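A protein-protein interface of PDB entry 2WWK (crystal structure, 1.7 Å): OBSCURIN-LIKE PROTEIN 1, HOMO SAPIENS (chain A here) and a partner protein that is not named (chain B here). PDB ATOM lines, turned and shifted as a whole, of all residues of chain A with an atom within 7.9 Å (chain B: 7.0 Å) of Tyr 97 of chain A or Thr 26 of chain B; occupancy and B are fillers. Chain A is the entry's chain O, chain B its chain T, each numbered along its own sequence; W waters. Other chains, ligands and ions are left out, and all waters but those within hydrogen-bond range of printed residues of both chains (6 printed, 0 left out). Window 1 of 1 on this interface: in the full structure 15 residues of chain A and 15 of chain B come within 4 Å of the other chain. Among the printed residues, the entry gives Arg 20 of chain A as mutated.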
ATOM      1  N   PRO A  14     -20.109  14.695   6.884  1.00  0.00           N
ATOM      2  CA  PRO A  14     -21.009  14.620   5.752  1.00  0.00           C
ATOM      3  C   PRO A  14     -20.262  14.350   4.445  1.00  0.00           C
ATOM      4  O   PRO A  14     -19.034  14.572   4.362  1.00  0.00           O
ATOM      5  CB  PRO A  14     -21.661  15.997   5.741  1.00  0.00           C
ATOM      6  CG  PRO A  14     -20.622  16.914   6.334  1.00  0.00           C
ATOM      7  CD  PRO A  14     -19.897  16.080   7.364  1.00  0.00           C
ATOM      8  N   PRO A  15     -20.992  13.925   3.402  1.00  0.00           N
ATOM      9  CA  PRO A  15     -20.333  13.653   2.129  1.00  0.00           C
ATOM     10  C   PRO A  15     -19.722  14.898   1.485  1.00  0.00           C
ATOM     11  O   PRO A  15     -20.266  15.983   1.545  1.00  0.00           O
ATOM     12  CB  PRO A  15     -21.465  13.108   1.235  1.00  0.00           C
ATOM     13  CG  PRO A  15     -22.530  12.599   2.232  1.00  0.00           C
ATOM     14  CD  PRO A  15     -22.421  13.583   3.388  1.00  0.00           C
ATOM     15  N   CYS A  16     -18.581  14.703   0.840  1.00  0.00           N
ATOM     16  CA  CYS A  16     -17.979  15.741   0.013  1.00  0.00           C
ATOM     17  C   CYS A  16     -17.426  15.117  -1.233  1.00  0.00           C
ATOM     18  O   CYS A  16     -17.086  13.941  -1.247  1.00  0.00           O
ATOM     19  CB  CYS A  16     -16.875  16.498   0.757  1.00  0.00           C
ATOM     20  SG  CYS A  16     -15.606  15.417   1.388  1.00  0.00           S
ATOM     21  N   PHE A  17     -17.348  15.911  -2.295  1.00  0.00           N
ATOM     22  CA  PHE A  17     -16.744  15.454  -3.520  1.00  0.00           C
ATOM     23  C   PHE A  17     -15.266  15.852  -3.586  1.00  0.00           C
ATOM     24  O   PHE A  17     -14.914  17.005  -3.313  1.00  0.00           O
ATOM     25  CB  PHE A  17     -17.451  16.044  -4.749  1.00  0.00           C
ATOM     26  CG  PHE A  17     -18.884  15.597  -4.921  1.00  0.00           C
ATOM     27  CD1 PHE A  17     -19.182  14.372  -5.479  1.00  0.00           C
ATOM     28  CD2 PHE A  17     -19.926  16.443  -4.567  1.00  0.00           C
ATOM     29  CE1 PHE A  17     -20.515  13.949  -5.650  1.00  0.00           C
ATOM     30  CE2 PHE A  17     -21.270  16.040  -4.744  1.00  0.00           C
ATOM     31  CZ  PHE A  17     -21.554  14.801  -5.273  1.00  0.00           C
ATOM     32  N   ARG A  20     -15.942  15.457  -9.276  1.00  0.00           N
ATOM     33  CA  ARG A  20     -17.296  15.582  -9.604  1.00  0.00           C
ATOM     34  C   ARG A  20     -17.507  15.072 -11.016  1.00  0.00           C
ATOM     35  O   ARG A  20     -16.560  15.078 -11.820  1.00  0.00           O
ATOM     36  CB  ARG A  20     -17.710  17.057  -9.476  1.00  0.00           C
ATOM     37  CG  ARG A  20     -17.871  17.425  -7.942  1.00  0.00           C
ATOM     38  CD  ARG A  20     -17.538  18.855  -7.609  1.00  0.00           C
ATOM     39  NE  ARG A  20     -16.179  19.034  -8.065  1.00  0.00           N
ATOM     40  CZ  ARG A  20     -15.088  18.966  -7.307  1.00  0.00           C
ATOM     41  NH1 ARG A  20     -15.157  18.845  -5.975  1.00  0.00           N
ATOM     42  NH2 ARG A  20     -13.925  19.045  -7.908  1.00  0.00           N
ATOM     43  N   PRO A  21     -18.729  14.654 -11.329  1.00  0.00           N
ATOM     44  CA  PRO A  21     -18.990  14.199 -12.688  1.00  0.00           C
ATOM     45  C   PRO A  21     -18.812  15.320 -13.691  1.00  0.00           C
ATOM     46  O   PRO A  21     -19.168  16.465 -13.389  1.00  0.00           O
ATOM     47  CB  PRO A  21     -20.438  13.715 -12.626  1.00  0.00           C
ATOM     48  CG  PRO A  21     -21.017  14.317 -11.443  1.00  0.00           C
ATOM     49  CD  PRO A  21     -19.917  14.518 -10.455  1.00  0.00           C
ATOM     50  N   VAL A  47     -26.172   7.429  -5.421  1.00  0.00           N
ATOM     51  CA  VAL A  47     -27.181   7.097  -6.375  1.00  0.00           C
ATOM     52  C   VAL A  47     -27.150   8.152  -7.458  1.00  0.00           C
ATOM     53  O   VAL A  47     -26.625   9.222  -7.237  1.00  0.00           O
ATOM     54  CB  VAL A  47     -28.607   6.997  -5.728  1.00  0.00           C
ATOM     55  CG1 VAL A  47     -28.641   5.969  -4.583  1.00  0.00           C
ATOM     56  CG2 VAL A  47     -29.092   8.321  -5.226  1.00  0.00           C
ATOM     57  N   GLU A  49     -29.516  10.196 -10.538  1.00  0.00           N
ATOM     58  CA  GLU A  49     -30.886  10.574 -10.856  1.00  0.00           C
ATOM     59  C   GLU A  49     -30.907  11.215 -12.217  1.00  0.00           C
ATOM     60  O   GLU A  49     -29.969  11.914 -12.602  1.00  0.00           O
ATOM     61  CB  GLU A  49     -31.459  11.518  -9.796  1.00  0.00           C
ATOM     62  CG  GLU A  49     -31.486  10.912  -8.396  1.00  0.00           C
ATOM     63  CD  GLU A  49     -31.859  11.902  -7.278  1.00  0.00           C
ATOM     64  OE1 GLU A  49     -31.939  13.136  -7.522  1.00  0.00           O
ATOM     65  OE2 GLU A  49     -32.082  11.408  -6.145  1.00  0.00           O
ATOM     66  N   VAL A  86     -27.718  13.497 -12.182  1.00  0.00           N
ATOM     67  CA  VAL A  86     -27.397  14.101 -10.893  1.00  0.00           C
ATOM     68  C   VAL A  86     -26.820  12.970 -10.052  1.00  0.00           C
ATOM     69  O   VAL A  86     -27.429  11.908  -9.905  1.00  0.00           O
ATOM     70  CB  VAL A  86     -28.615  14.708 -10.218  1.00  0.00           C
ATOM     71  CG1 VAL A  86     -28.262  15.186  -8.806  1.00  0.00           C
ATOM     72  CG2 VAL A  86     -29.172  15.862 -11.071  1.00  0.00           C
ATOM     73  N   CYS A  87     -25.677  13.243  -9.443  1.00  0.00           N
ATOM     74  CA  CYS A  87     -25.004  12.346  -8.532  1.00  0.00           C
ATOM     75  C   CYS A  87     -25.322  12.812  -7.114  1.00  0.00           C
ATOM     76  O   CYS A  87     -25.130  13.975  -6.793  1.00  0.00           O
ATOM     77  CB  CYS A  87     -23.478  12.404  -8.789  1.00  0.00           C
ATOM     78  SG  CYS A  87     -22.532  11.415  -7.665  1.00  0.00           S
ATOM     79  N   ARG A  88     -25.911  11.926  -6.324  1.00  0.00           N
ATOM     80  CA  ARG A  88     -26.371  12.229  -4.957  1.00  0.00           C
ATOM     81  C   ARG A  88     -25.671  11.294  -4.034  1.00  0.00           C
ATOM     82  O   ARG A  88     -25.878  10.080  -4.071  1.00  0.00           O
ATOM     83  CB  ARG A  88     -27.884  12.051  -4.846  1.00  0.00           C
ATOM     84  CG  ARG A  88     -28.491  12.236  -3.461  1.00  0.00           C
ATOM     85  CD  ARG A  88     -29.961  11.908  -3.491  1.00  0.00           C
ATOM     86  NE  ARG A  88     -30.626  12.265  -2.257  1.00  0.00           N
ATOM     87  CZ  ARG A  88     -31.901  12.016  -2.015  1.00  0.00           C
ATOM     88  NH1 ARG A  88     -32.657  11.414  -2.934  1.00  0.00           N
ATOM     89  NH2 ARG A  88     -32.429  12.396  -0.863  1.00  0.00           N
ATOM     90  N   ALA A  89     -24.864  11.881  -3.148  1.00  0.00           N
ATOM     91  CA  ALA A  89     -24.103  11.079  -2.181  1.00  0.00           C
ATOM     92  C   ALA A  89     -24.679  11.339  -0.789  1.00  0.00           C
ATOM     93  O   ALA A  89     -24.914  12.498  -0.459  1.00  0.00           O
ATOM     94  CB  ALA A  89     -22.644  11.511  -2.244  1.00  0.00           C
ATOM     95  N   ARG A  90     -24.924  10.284   0.003  1.00  0.00           N
ATOM     96  CA  ARG A  90     -25.695  10.400   1.254  1.00  0.00           C
ATOM     97  C   ARG A  90     -25.062   9.564   2.365  1.00  0.00           C
ATOM     98  O   ARG A  90     -24.606   8.451   2.129  1.00  0.00           O
ATOM     99  CB  ARG A  90     -27.122   9.893   0.973  1.00  0.00           C
ATOM    100  CG  ARG A  90     -28.234  10.145   1.943  1.00  0.00           C
ATOM    101  CD  ARG A  90     -29.582  10.304   1.113  1.00  0.00           C
ATOM    102  NE  ARG A  90     -29.645   9.510  -0.143  1.00  0.00           N
ATOM    103  CZ  ARG A  90     -30.702   8.772  -0.535  1.00  0.00           C
ATOM    104  NH1 ARG A  90     -31.821   8.741   0.186  1.00  0.00           N
ATOM    105  NH2 ARG A  90     -30.656   8.076  -1.681  1.00  0.00           N
ATOM    106  N   GLY A  94     -25.232  13.980   6.199  1.00  0.00           N
ATOM    107  CA  GLY A  94     -25.645  14.907   5.151  1.00  0.00           C
ATOM    108  C   GLY A  94     -25.672  14.323   3.752  1.00  0.00           C
ATOM    109  O   GLY A  94     -25.591  13.123   3.558  1.00  0.00           O
ATOM    110  N   GLU A  95     -25.848  15.206   2.780  1.00  0.00           N
ATOM    111  CA  GLU A  95     -25.938  14.842   1.384  1.00  0.00           C
ATOM    112  C   GLU A  95     -25.108  15.806   0.588  1.00  0.00           C
ATOM    113  O   GLU A  95     -24.947  16.986   1.002  1.00  0.00           O
ATOM    114  CB  GLU A  95     -27.389  14.827   0.903  1.00  0.00           C
ATOM    115  CG  GLU A  95     -28.334  14.069   1.842  1.00  0.00           C
ATOM    116  CD  GLU A  95     -29.737  13.776   1.300  1.00  0.00           C
ATOM    117  OE1 GLU A  95     -30.685  13.682   2.128  1.00  0.00           O
ATOM    118  OE2 GLU A  95     -29.914  13.618   0.096  1.00  0.00           O
ATOM    119  N   ALA A  96     -24.576  15.320  -0.526  1.00  0.00           N
ATOM    120  CA  ALA A  96     -23.895  16.170  -1.491  1.00  0.00           C
ATOM    121  C   ALA A  96     -24.443  15.863  -2.874  1.00  0.00           C
ATOM    122  O   ALA A  96     -24.726  14.687  -3.191  1.00  0.00           O
ATOM    123  CB  ALA A  96     -22.372  15.999  -1.443  1.00  0.00           C
ATOM    124  N   TYR A  97     -24.568  16.914  -3.679  1.00  0.00           N
ATOM    125  CA  TYR A  97     -25.083  16.794  -5.029  1.00  0.00           C
ATOM    126  C   TYR A  97     -24.183  17.465  -6.075  1.00  0.00           C
ATOM    127  O   TYR A  97     -23.677  18.537  -5.846  1.00  0.00           O
ATOM    128  CB  TYR A  97     -26.444  17.422  -5.144  1.00  0.00           C
ATOM    129  CG  TYR A  97     -27.557  16.813  -4.371  1.00  0.00           C
ATOM    130  CD1 TYR A  97     -28.540  16.070  -5.021  1.00  0.00           C
ATOM    131  CD2 TYR A  97     -27.706  17.050  -3.005  1.00  0.00           C
ATOM    132  CE1 TYR A  97     -29.629  15.564  -4.327  1.00  0.00           C
ATOM    133  CE2 TYR A  97     -28.799  16.519  -2.284  1.00  0.00           C
ATOM    134  CZ  TYR A  97     -29.750  15.761  -2.952  1.00  0.00           C
ATOM    135  OH  TYR A  97     -30.839  15.260  -2.239  1.00  0.00           O
ATOM    136  N   ALA A  98     -24.035  16.799  -7.239  1.00  0.00           N
ATOM    137  CA  ALA A  98     -23.325  17.387  -8.365  1.00  0.00           C
ATOM    138  C   ALA A  98     -23.917  16.774  -9.626  1.00  0.00           C
ATOM    139  O   ALA A  98     -24.314  15.621  -9.639  1.00  0.00           O
ATOM    140  CB  ALA A  98     -21.847  17.103  -8.267  1.00  0.00           C
ATOM    141  N   ALA A  99     -24.000  17.553 -10.678  1.00  0.00           N
ATOM    142  CA  ALA A  99     -24.682  17.126 -11.907  1.00  0.00           C
ATOM    143  C   ALA A  99     -23.747  17.255 -13.104  1.00  0.00           C
ATOM    144  O   ALA A  99     -22.734  17.966 -13.071  1.00  0.00           O
ATOM    145  CB  ALA A  99     -25.935  17.973 -12.141  1.00  0.00           C
ATOM    146  N   LEU B  13     -26.748  21.738 -13.170  1.00  0.00           N
ATOM    147  CA  LEU B  13     -27.082  22.034 -11.813  1.00  0.00           C
ATOM    148  C   LEU B  13     -28.384  21.318 -11.566  1.00  0.00           C
ATOM    149  O   LEU B  13     -29.317  21.490 -12.341  1.00  0.00           O
ATOM    150  CB  LEU B  13     -27.258  23.542 -11.574  1.00  0.00           C
ATOM    151  CG  LEU B  13     -27.662  24.015 -10.149  1.00  0.00           C
ATOM    152  CD1 LEU B  13     -26.513  23.864  -9.145  1.00  0.00           C
ATOM    153  CD2 LEU B  13     -28.181  25.454 -10.126  1.00  0.00           C
ATOM    154  N   PRO B  14     -28.484  20.557 -10.469  1.00  0.00           N
ATOM    155  CA  PRO B  14     -29.772  19.916 -10.193  1.00  0.00           C
ATOM    156  C   PRO B  14     -30.935  20.904 -10.146  1.00  0.00           C
ATOM    157  O   PRO B  14     -30.757  21.987  -9.667  1.00  0.00           O
ATOM    158  CB  PRO B  14     -29.551  19.285  -8.814  1.00  0.00           C
ATOM    159  CG  PRO B  14     -28.090  19.234  -8.644  1.00  0.00           C
ATOM    160  CD  PRO B  14     -27.501  20.329  -9.385  1.00  0.00           C
ATOM    161  N   ASP B  16     -33.874  20.261  -8.470  1.00  0.00           N
ATOM    162  CA  ASP B  16     -34.439  20.050  -7.123  1.00  0.00           C
ATOM    163  C   ASP B  16     -33.522  19.164  -6.292  1.00  0.00           C
ATOM    164  O   ASP B  16     -32.937  18.172  -6.797  1.00  0.00           O
ATOM    165  CB  ASP B  16     -35.791  19.383  -7.190  1.00  0.00           C
ATOM    166  CG  ASP B  16     -36.834  20.233  -7.825  1.00  0.00           C
ATOM    167  OD1 ASP B  16     -37.568  20.912  -7.071  1.00  0.00           O
ATOM    168  OD2 ASP B  16     -36.942  20.212  -9.079  1.00  0.00           O
ATOM    169  N   ILE B  17     -33.354  19.534  -5.026  1.00  0.00           N
ATOM    170  CA  ILE B  17     -32.579  18.731  -4.088  1.00  0.00           C
ATOM    171  C   ILE B  17     -33.300  18.718  -2.760  1.00  0.00           C
ATOM    172  O   ILE B  17     -34.112  19.604  -2.481  1.00  0.00           O
ATOM    173  CB  ILE B  17     -31.096  19.172  -3.942  1.00  0.00           C
ATOM    174  CG1 ILE B  17     -30.935  20.606  -3.478  1.00  0.00           C
ATOM    175  CG2 ILE B  17     -30.311  19.013  -5.275  1.00  0.00           C
ATOM    176  CD1 ILE B  17     -29.458  20.996  -3.328  1.00  0.00           C
ATOM    177  N   SER B  18     -33.013  17.686  -1.968  1.00  0.00           N
ATOM    178  CA  SER B  18     -33.652  17.446  -0.660  1.00  0.00           C
ATOM    179  C   SER B  18     -32.602  17.151   0.377  1.00  0.00           C
ATOM    180  O   SER B  18     -31.548  16.554   0.068  1.00  0.00           O
ATOM    181  CB  SER B  18     -34.595  16.267  -0.703  1.00  0.00           C
ATOM    182  OG  SER B  18     -35.762  16.572  -1.450  1.00  0.00           O
ATOM    183  N   ILE B  19     -32.894  17.569   1.613  1.00  0.00           N
ATOM    184  CA  ILE B  19     -32.017  17.348   2.723  1.00  0.00           C
ATOM    185  C   ILE B  19     -32.945  17.274   3.956  1.00  0.00           C
ATOM    186  O   ILE B  19     -33.966  17.941   4.005  1.00  0.00           O
ATOM    187  CB  ILE B  19     -30.981  18.493   2.842  1.00  0.00           C
ATOM    188  CG1 ILE B  19     -29.992  18.267   4.002  1.00  0.00           C
ATOM    189  CG2 ILE B  19     -31.705  19.844   2.985  1.00  0.00           C
ATOM    190  CD1 ILE B  19     -28.927  17.222   3.674  1.00  0.00           C
ATOM    191  N   VAL B  24     -26.217  18.337   7.001  1.00  0.00           N
ATOM    192  CA  VAL B  24     -25.411  19.209   6.152  1.00  0.00           C
ATOM    193  C   VAL B  24     -25.682  18.945   4.642  1.00  0.00           C
ATOM    194  O   VAL B  24     -25.692  17.785   4.189  1.00  0.00           O
ATOM    195  CB  VAL B  24     -23.941  18.973   6.403  1.00  0.00           C
ATOM    196  CG1 VAL B  24     -23.085  19.857   5.478  1.00  0.00           C
ATOM    197  CG2 VAL B  24     -23.608  19.167   7.887  1.00  0.00           C
ATOM    198  N   LEU B  25     -25.843  20.009   3.870  1.00  0.00           N
ATOM    199  CA  LEU B  25     -26.132  19.917   2.451  1.00  0.00           C
ATOM    200  C   LEU B  25     -25.012  20.556   1.679  1.00  0.00           C
ATOM    201  O   LEU B  25     -24.649  21.701   1.962  1.00  0.00           O
ATOM    202  CB  LEU B  25     -27.405  20.660   2.115  1.00  0.00           C
ATOM    203  CG  LEU B  25     -27.759  20.689   0.620  1.00  0.00           C
ATOM    204  CD1 LEU B  25     -27.975  19.315  -0.021  1.00  0.00           C
ATOM    205  CD2 LEU B  25     -28.966  21.568   0.370  1.00  0.00           C
ATOM    206  N   THR B  26     -24.509  19.850   0.673  1.00  0.00           N
ATOM    207  CA  THR B  26     -23.469  20.385  -0.191  1.00  0.00           C
ATOM    208  C   THR B  26     -23.968  20.334  -1.635  1.00  0.00           C
ATOM    209  O   THR B  26     -24.501  19.304  -2.056  1.00  0.00           O
ATOM    210  CB  THR B  26     -22.173  19.583  -0.033  1.00  0.00           C
ATOM    211  OG1 THR B  26     -21.706  19.644   1.327  1.00  0.00           O
ATOM    212  CG2 THR B  26     -21.103  20.125  -0.965  1.00  0.00           C
ATOM    213  N   VAL B  27     -23.837  21.430  -2.367  1.00  0.00           N
ATOM    214  CA  VAL B  27     -24.126  21.456  -3.822  1.00  0.00           C
ATOM    215  C   VAL B  27     -22.923  22.025  -4.545  1.00  0.00           C
ATOM    216  O   VAL B  27     -22.460  23.078  -4.198  1.00  0.00           O
ATOM    217  CB  VAL B  27     -25.318  22.316  -4.157  1.00  0.00           C
ATOM    218  CG1 VAL B  27     -25.710  22.074  -5.644  1.00  0.00           C
ATOM    219  CG2 VAL B  27     -26.452  22.017  -3.229  1.00  0.00           C
ATOM    220  N   ALA B  28     -22.405  21.291  -5.519  1.00  0.00           N
ATOM    221  CA  ALA B  28     -21.280  21.752  -6.298  1.00  0.00           C
ATOM    222  C   ALA B  28     -21.730  21.939  -7.739  1.00  0.00           C
ATOM    223  O   ALA B  28     -22.471  21.102  -8.288  1.00  0.00           O
ATOM    224  CB  ALA B  28     -20.172  20.762  -6.229  1.00  0.00           C
ATOM    225  N   CYS B  29     -21.192  22.958  -8.395  1.00  0.00           N
ATOM    226  CA  CYS B  29     -21.534  23.262  -9.763  1.00  0.00           C
ATOM    227  C   CYS B  29     -20.304  23.872 -10.453  1.00  0.00           C
ATOM    228  O   CYS B  29     -19.667  24.763  -9.937  1.00  0.00           O
ATOM    229  CB  CYS B  29     -22.716  24.249  -9.827  1.00  0.00           C
ATOM    230  SG  CYS B  29     -23.445  24.500 -11.460  1.00  0.00           S
ATOM    231  N   GLU B  59     -17.312  28.056  -1.366  1.00  0.00           N
ATOM    232  CA  GLU B  59     -15.937  27.859  -1.828  1.00  0.00           C
ATOM    233  C   GLU B  59     -15.909  27.948  -3.346  1.00  0.00           C
ATOM    234  O   GLU B  59     -16.546  27.137  -4.072  1.00  0.00           O
ATOM    235  CB  GLU B  59     -15.395  26.489  -1.389  1.00  0.00           C
ATOM    236  CG  GLU B  59     -15.151  26.311   0.084  1.00  0.00           C
ATOM    237  CD  GLU B  59     -16.371  25.805   0.915  1.00  0.00           C
ATOM    238  OE1 GLU B  59     -17.463  25.492   0.348  1.00  0.00           O
ATOM    239  OE2 GLU B  59     -16.212  25.714   2.171  1.00  0.00           O
ATOM    240  N   THR B  66     -18.875  25.608  -4.689  1.00  0.00           N
ATOM    241  CA  THR B  66     -19.518  24.680  -3.766  1.00  0.00           C
ATOM    242  C   THR B  66     -20.174  25.454  -2.662  1.00  0.00           C
ATOM    243  O   THR B  66     -19.506  26.221  -1.969  1.00  0.00           O
ATOM    244  CB  THR B  66     -18.518  23.636  -3.198  1.00  0.00           C
ATOM    245  OG1 THR B  66     -17.791  23.033  -4.280  1.00  0.00           O
ATOM    246  CG2 THR B  66     -19.244  22.535  -2.361  1.00  0.00           C
ATOM    247  N   LEU B  67     -21.463  25.211  -2.486  1.00  0.00           N
ATOM    248  CA  LEU B  67     -22.270  25.789  -1.453  1.00  0.00           C
ATOM    249  C   LEU B  67     -22.558  24.730  -0.403  1.00  0.00           C
ATOM    250  O   LEU B  67     -23.013  23.633  -0.715  1.00  0.00           O
ATOM    251  CB  LEU B  67     -23.578  26.276  -2.035  1.00  0.00           C
ATOM    252  CG  LEU B  67     -24.694  26.704  -1.048  1.00  0.00           C
ATOM    253  CD1 LEU B  67     -24.239  27.964  -0.213  1.00  0.00           C
ATOM    254  CD2 LEU B  67     -26.028  26.968  -1.745  1.00  0.00           C
ATOM    255  N   ILE B  68     -22.285  25.068   0.843  1.00  0.00           N
ATOM    256  CA  ILE B  68     -22.538  24.183   1.968  1.00  0.00           C
ATOM    257  C   ILE B  68     -23.434  24.883   2.955  1.00  0.00           C
ATOM    258  O   ILE B  68     -23.180  26.048   3.311  1.00  0.00           O
ATOM    259  CB  ILE B  68     -21.210  23.791   2.708  1.00  0.00           C
ATOM    260  CG1 ILE B  68     -20.291  23.031   1.753  1.00  0.00           C
ATOM    261  CG2 ILE B  68     -21.490  22.967   3.942  1.00  0.00           C
ATOM    262  CD1 ILE B  68     -18.896  22.834   2.261  1.00  0.00           C
ATOM    263  N   ILE B  69     -24.483  24.187   3.396  1.00  0.00           N
ATOM    264  CA  ILE B  69     -25.371  24.731   4.427  1.00  0.00           C
ATOM    265  C   ILE B  69     -25.330  23.720   5.556  1.00  0.00           C
ATOM    266  O   ILE B  69     -25.690  22.545   5.387  1.00  0.00           O
ATOM    267  CB  ILE B  69     -26.827  24.959   3.936  1.00  0.00           C
ATOM    268  CG1 ILE B  69     -26.842  25.731   2.601  1.00  0.00           C
ATOM    269  CG2 ILE B  69     -27.612  25.680   5.063  1.00  0.00           C
ATOM    270  CD1 ILE B  69     -28.208  25.903   1.954  1.00  0.00           C
ATOM    271  N   ARG B 100     -36.745  18.335   4.541  1.00  0.00           N
ATOM    272  CA  ARG B 100     -37.682  17.390   5.162  1.00  0.00           C
ATOM    273  C   ARG B 100     -37.621  17.434   6.683  1.00  0.00           C
ATOM    274  O   ARG B 100     -36.558  17.283   7.271  1.00  0.00           O
ATOM    275  CB  ARG B 100     -37.455  15.981   4.629  1.00  0.00           C
ATOM    276  CG  ARG B 100     -37.772  15.889   3.127  1.00  0.00           C
ATOM    277  CD  ARG B 100     -37.184  14.627   2.479  1.00  0.00           C
ATOM    278  NE  ARG B 100     -35.720  14.650   2.492  1.00  0.00           N
ATOM    279  CZ  ARG B 100     -34.939  13.814   1.806  1.00  0.00           C
ATOM    280  NH1 ARG B 100     -35.471  12.864   1.036  1.00  0.00           N
ATOM    281  NH2 ARG B 100     -33.613  13.934   1.889  1.00  0.00           N
HETATM  282  O   HOH W   1     -35.376  11.405  -1.225  1.00  0.00           O
HETATM  283  O   HOH W   2     -31.716  16.056  -7.538  1.00  0.00           O
HETATM  284  O   HOH W   3     -19.117  18.986   1.846  1.00  0.00           O
HETATM  285  O   HOH W   4     -22.544  17.244   2.487  1.00  0.00           O
HETATM  286  O   HOH W   5     -17.038  20.314  -4.260  1.00  0.00           O
HETATM  287  O   HOH W   6     -24.213  20.492 -10.203  1.00  0.00           O
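N of Glu 95 of chain A sits at hydrogen-bond distance from O of Val 24 of chain B. The backbone carbonyl oxygen of Glu 95 of chain A is in hydrogen-bond range of the backbone NH of Thr 26 of chain B, 2.9 Å away. The side-chain carboxylate of Glu 95 of chain A is in salt-bridge range of the guanidinium group of Arg 100 of chain B, 2.9 Å away. O of Ser 18 of chain B is in hydrogen-bond range of OH of Tyr 97 of chain A (2.7 Å). The backbone carbonyl oxygen (O) of Thr 26 of chain B is in hydrogen-bond range of the backbone NH (N) of Tyr 97 of chain A, 2.9 Å away. O of Tyr 97 of chain A lies within hydrogen-bond range of N of Ala 28 of chain B (3.1 Å). NH2 of Arg 100 of chain B lies close to NH2 of Arg 88 of chain A (3.4 Å). The backbone carbonyl oxygen (O) of Ser 18 of chain B lies close to the side-chain carboxylate (OE2) of Glu 95 of chain A (3.4 Å).
Tyr 97 of chain A touches just these residues of chain B: Ile 17 (3.4 Å), Ser 18 (2.7 Å), Leu 25 (3.7 Å), Thr 26 (2.9 Å), Val 27 (3.6 Å) and Ala 28 (3.1 Å). Thr 26 of chain B touches four residues of chain A. Printed residues of chain A within 4 Å of Arg 100 of chain B: Arg 88 (3.4 Å) and Glu 95 (2.9 Å). Of the printed residues of chain B, Pro 15 of chain A touches Thr 26 (3.9 Å). Of the printed residues of chain A, Val 27 of chain B touches Tyr 97 (3.6 Å). Printed residues of chain B within 4 Å of Arg 88 of chain A: Arg 100 (3.4 Å). The nearest printed residue of chain A that does not touch Arg 100 of chain B is Tyr 97 of chain A (5.1 Å).
The guanidinium group (NH1) of Arg 88 of chain A is in salt-bridge range of the side-chain carboxylate (OE2) of Glu 49 of chain A, at 3.3 Å. The backbone NH (N) of Cys 87 of chain A lies within hydrogen-bond range of the backbone carbonyl oxygen (O) of Ala 98 of chain A (2.7 Å). NE of Arg 88 of chain A lies within salt-bridge range of OE2 of Glu 95 of chain A (2.8 Å). The side-chain hydroxyl (OH) of Tyr 97 of chain A is in hydrogen-bond range of the guanidinium group (NE) of Arg 88 of chain A (3.0 Å). The backbone carbonyl oxygen (O) of Ala 96 of chain A lies within hydrogen-bond range of the backbone NH (N) of Ala 89 of chain A, 2.8 Å away. The side-chain carboxylate (OE2) of Glu 95 of chain A sits at hydrogen-bond distance from the side-chain hydroxyl (OH) of Tyr 97 of chain A, at 3.0 Å.
Water W2 lies within hydrogen-bond range of the backbone carbonyl oxygen of Asp 16 of chain B (2.6 Å) and the side-chain carboxylate of Glu 49 of chain A (2.9 Å). Water W6 lies within hydrogen-bond range of O of Ala 28 of chain B (2.7 Å) and N of Ala 99 of chain A (3.0 Å). Water W1 bridges the guanidinium group (NH1) of Arg 100 of chain B (2.7 Å) and the guanidinium group (NH2) of Arg 88 of chain A (3.1 Å). Water W3 lies within hydrogen-bond range of the side-chain hydroxyl of Thr 26 of chain B (2.7 Å) and the backbone carbonyl oxygen of Pro 15 of chain A (3.2 Å). Water W4 lies within hydrogen-bond range of O of Pro 15 of chain A, OG1 of Thr 26 of chain B and O of Glu 95 of chain A. Water W5 bridges the side-chain hydroxyl of Thr 66 of chain B (2.8 Å) and the guanidinium group of Arg 20 of chain A (2.9 Å).
Printed residues of chain A that touch a printed residue of chain B: Pro 14, Pro 15, Arg 20, Arg 88, Gly 94, Glu 95, Ala 96, Tyr 97, Ala 98 and Ala 99. Of the 18 printed residues of chain B, 11 touch a printed residue of chain A. Hydrophobic or aromatic side chains of chain B that line the printed part of chain A: Pro 14, Ile 17, Ile 19, Val 24, Leu 25 and Ala 28. Among the printed residues, 21 pairs touch across the chains. Among the printed residues, Asp or Glu carboxylates within 4 Å of a Lys or Arg side-chain nitrogen of the other chain: Glu 95 of chain A with Arg 100 of chain B.
Pro 14 of chain A touches Val 24 of chain B. Thr 26 of chain B touches Pro 15 of chain A. Arg 20 of chain A touches Ala 28 of chain B. Gly 94 of chain A touches Val 24 of chain B. Glu 95 of chain A touches Leu 25 of chain B. CD1 of Tyr 97 of chain A touches CG2 of Ile 17 of chain B, 3.4 Å away. Tyr 97 of chain A touches Leu 25 of chain B. CA of Ala 98 of chain A touches O of Ala 28 of chain B, 3.8 Å away. Ala 99 of chain A touches Leu 13 of chain B (CB to N, 3.99 Å). Ala 99 of chain A touches Pro 14 of chain B (CB to CD, 3.9 Å).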
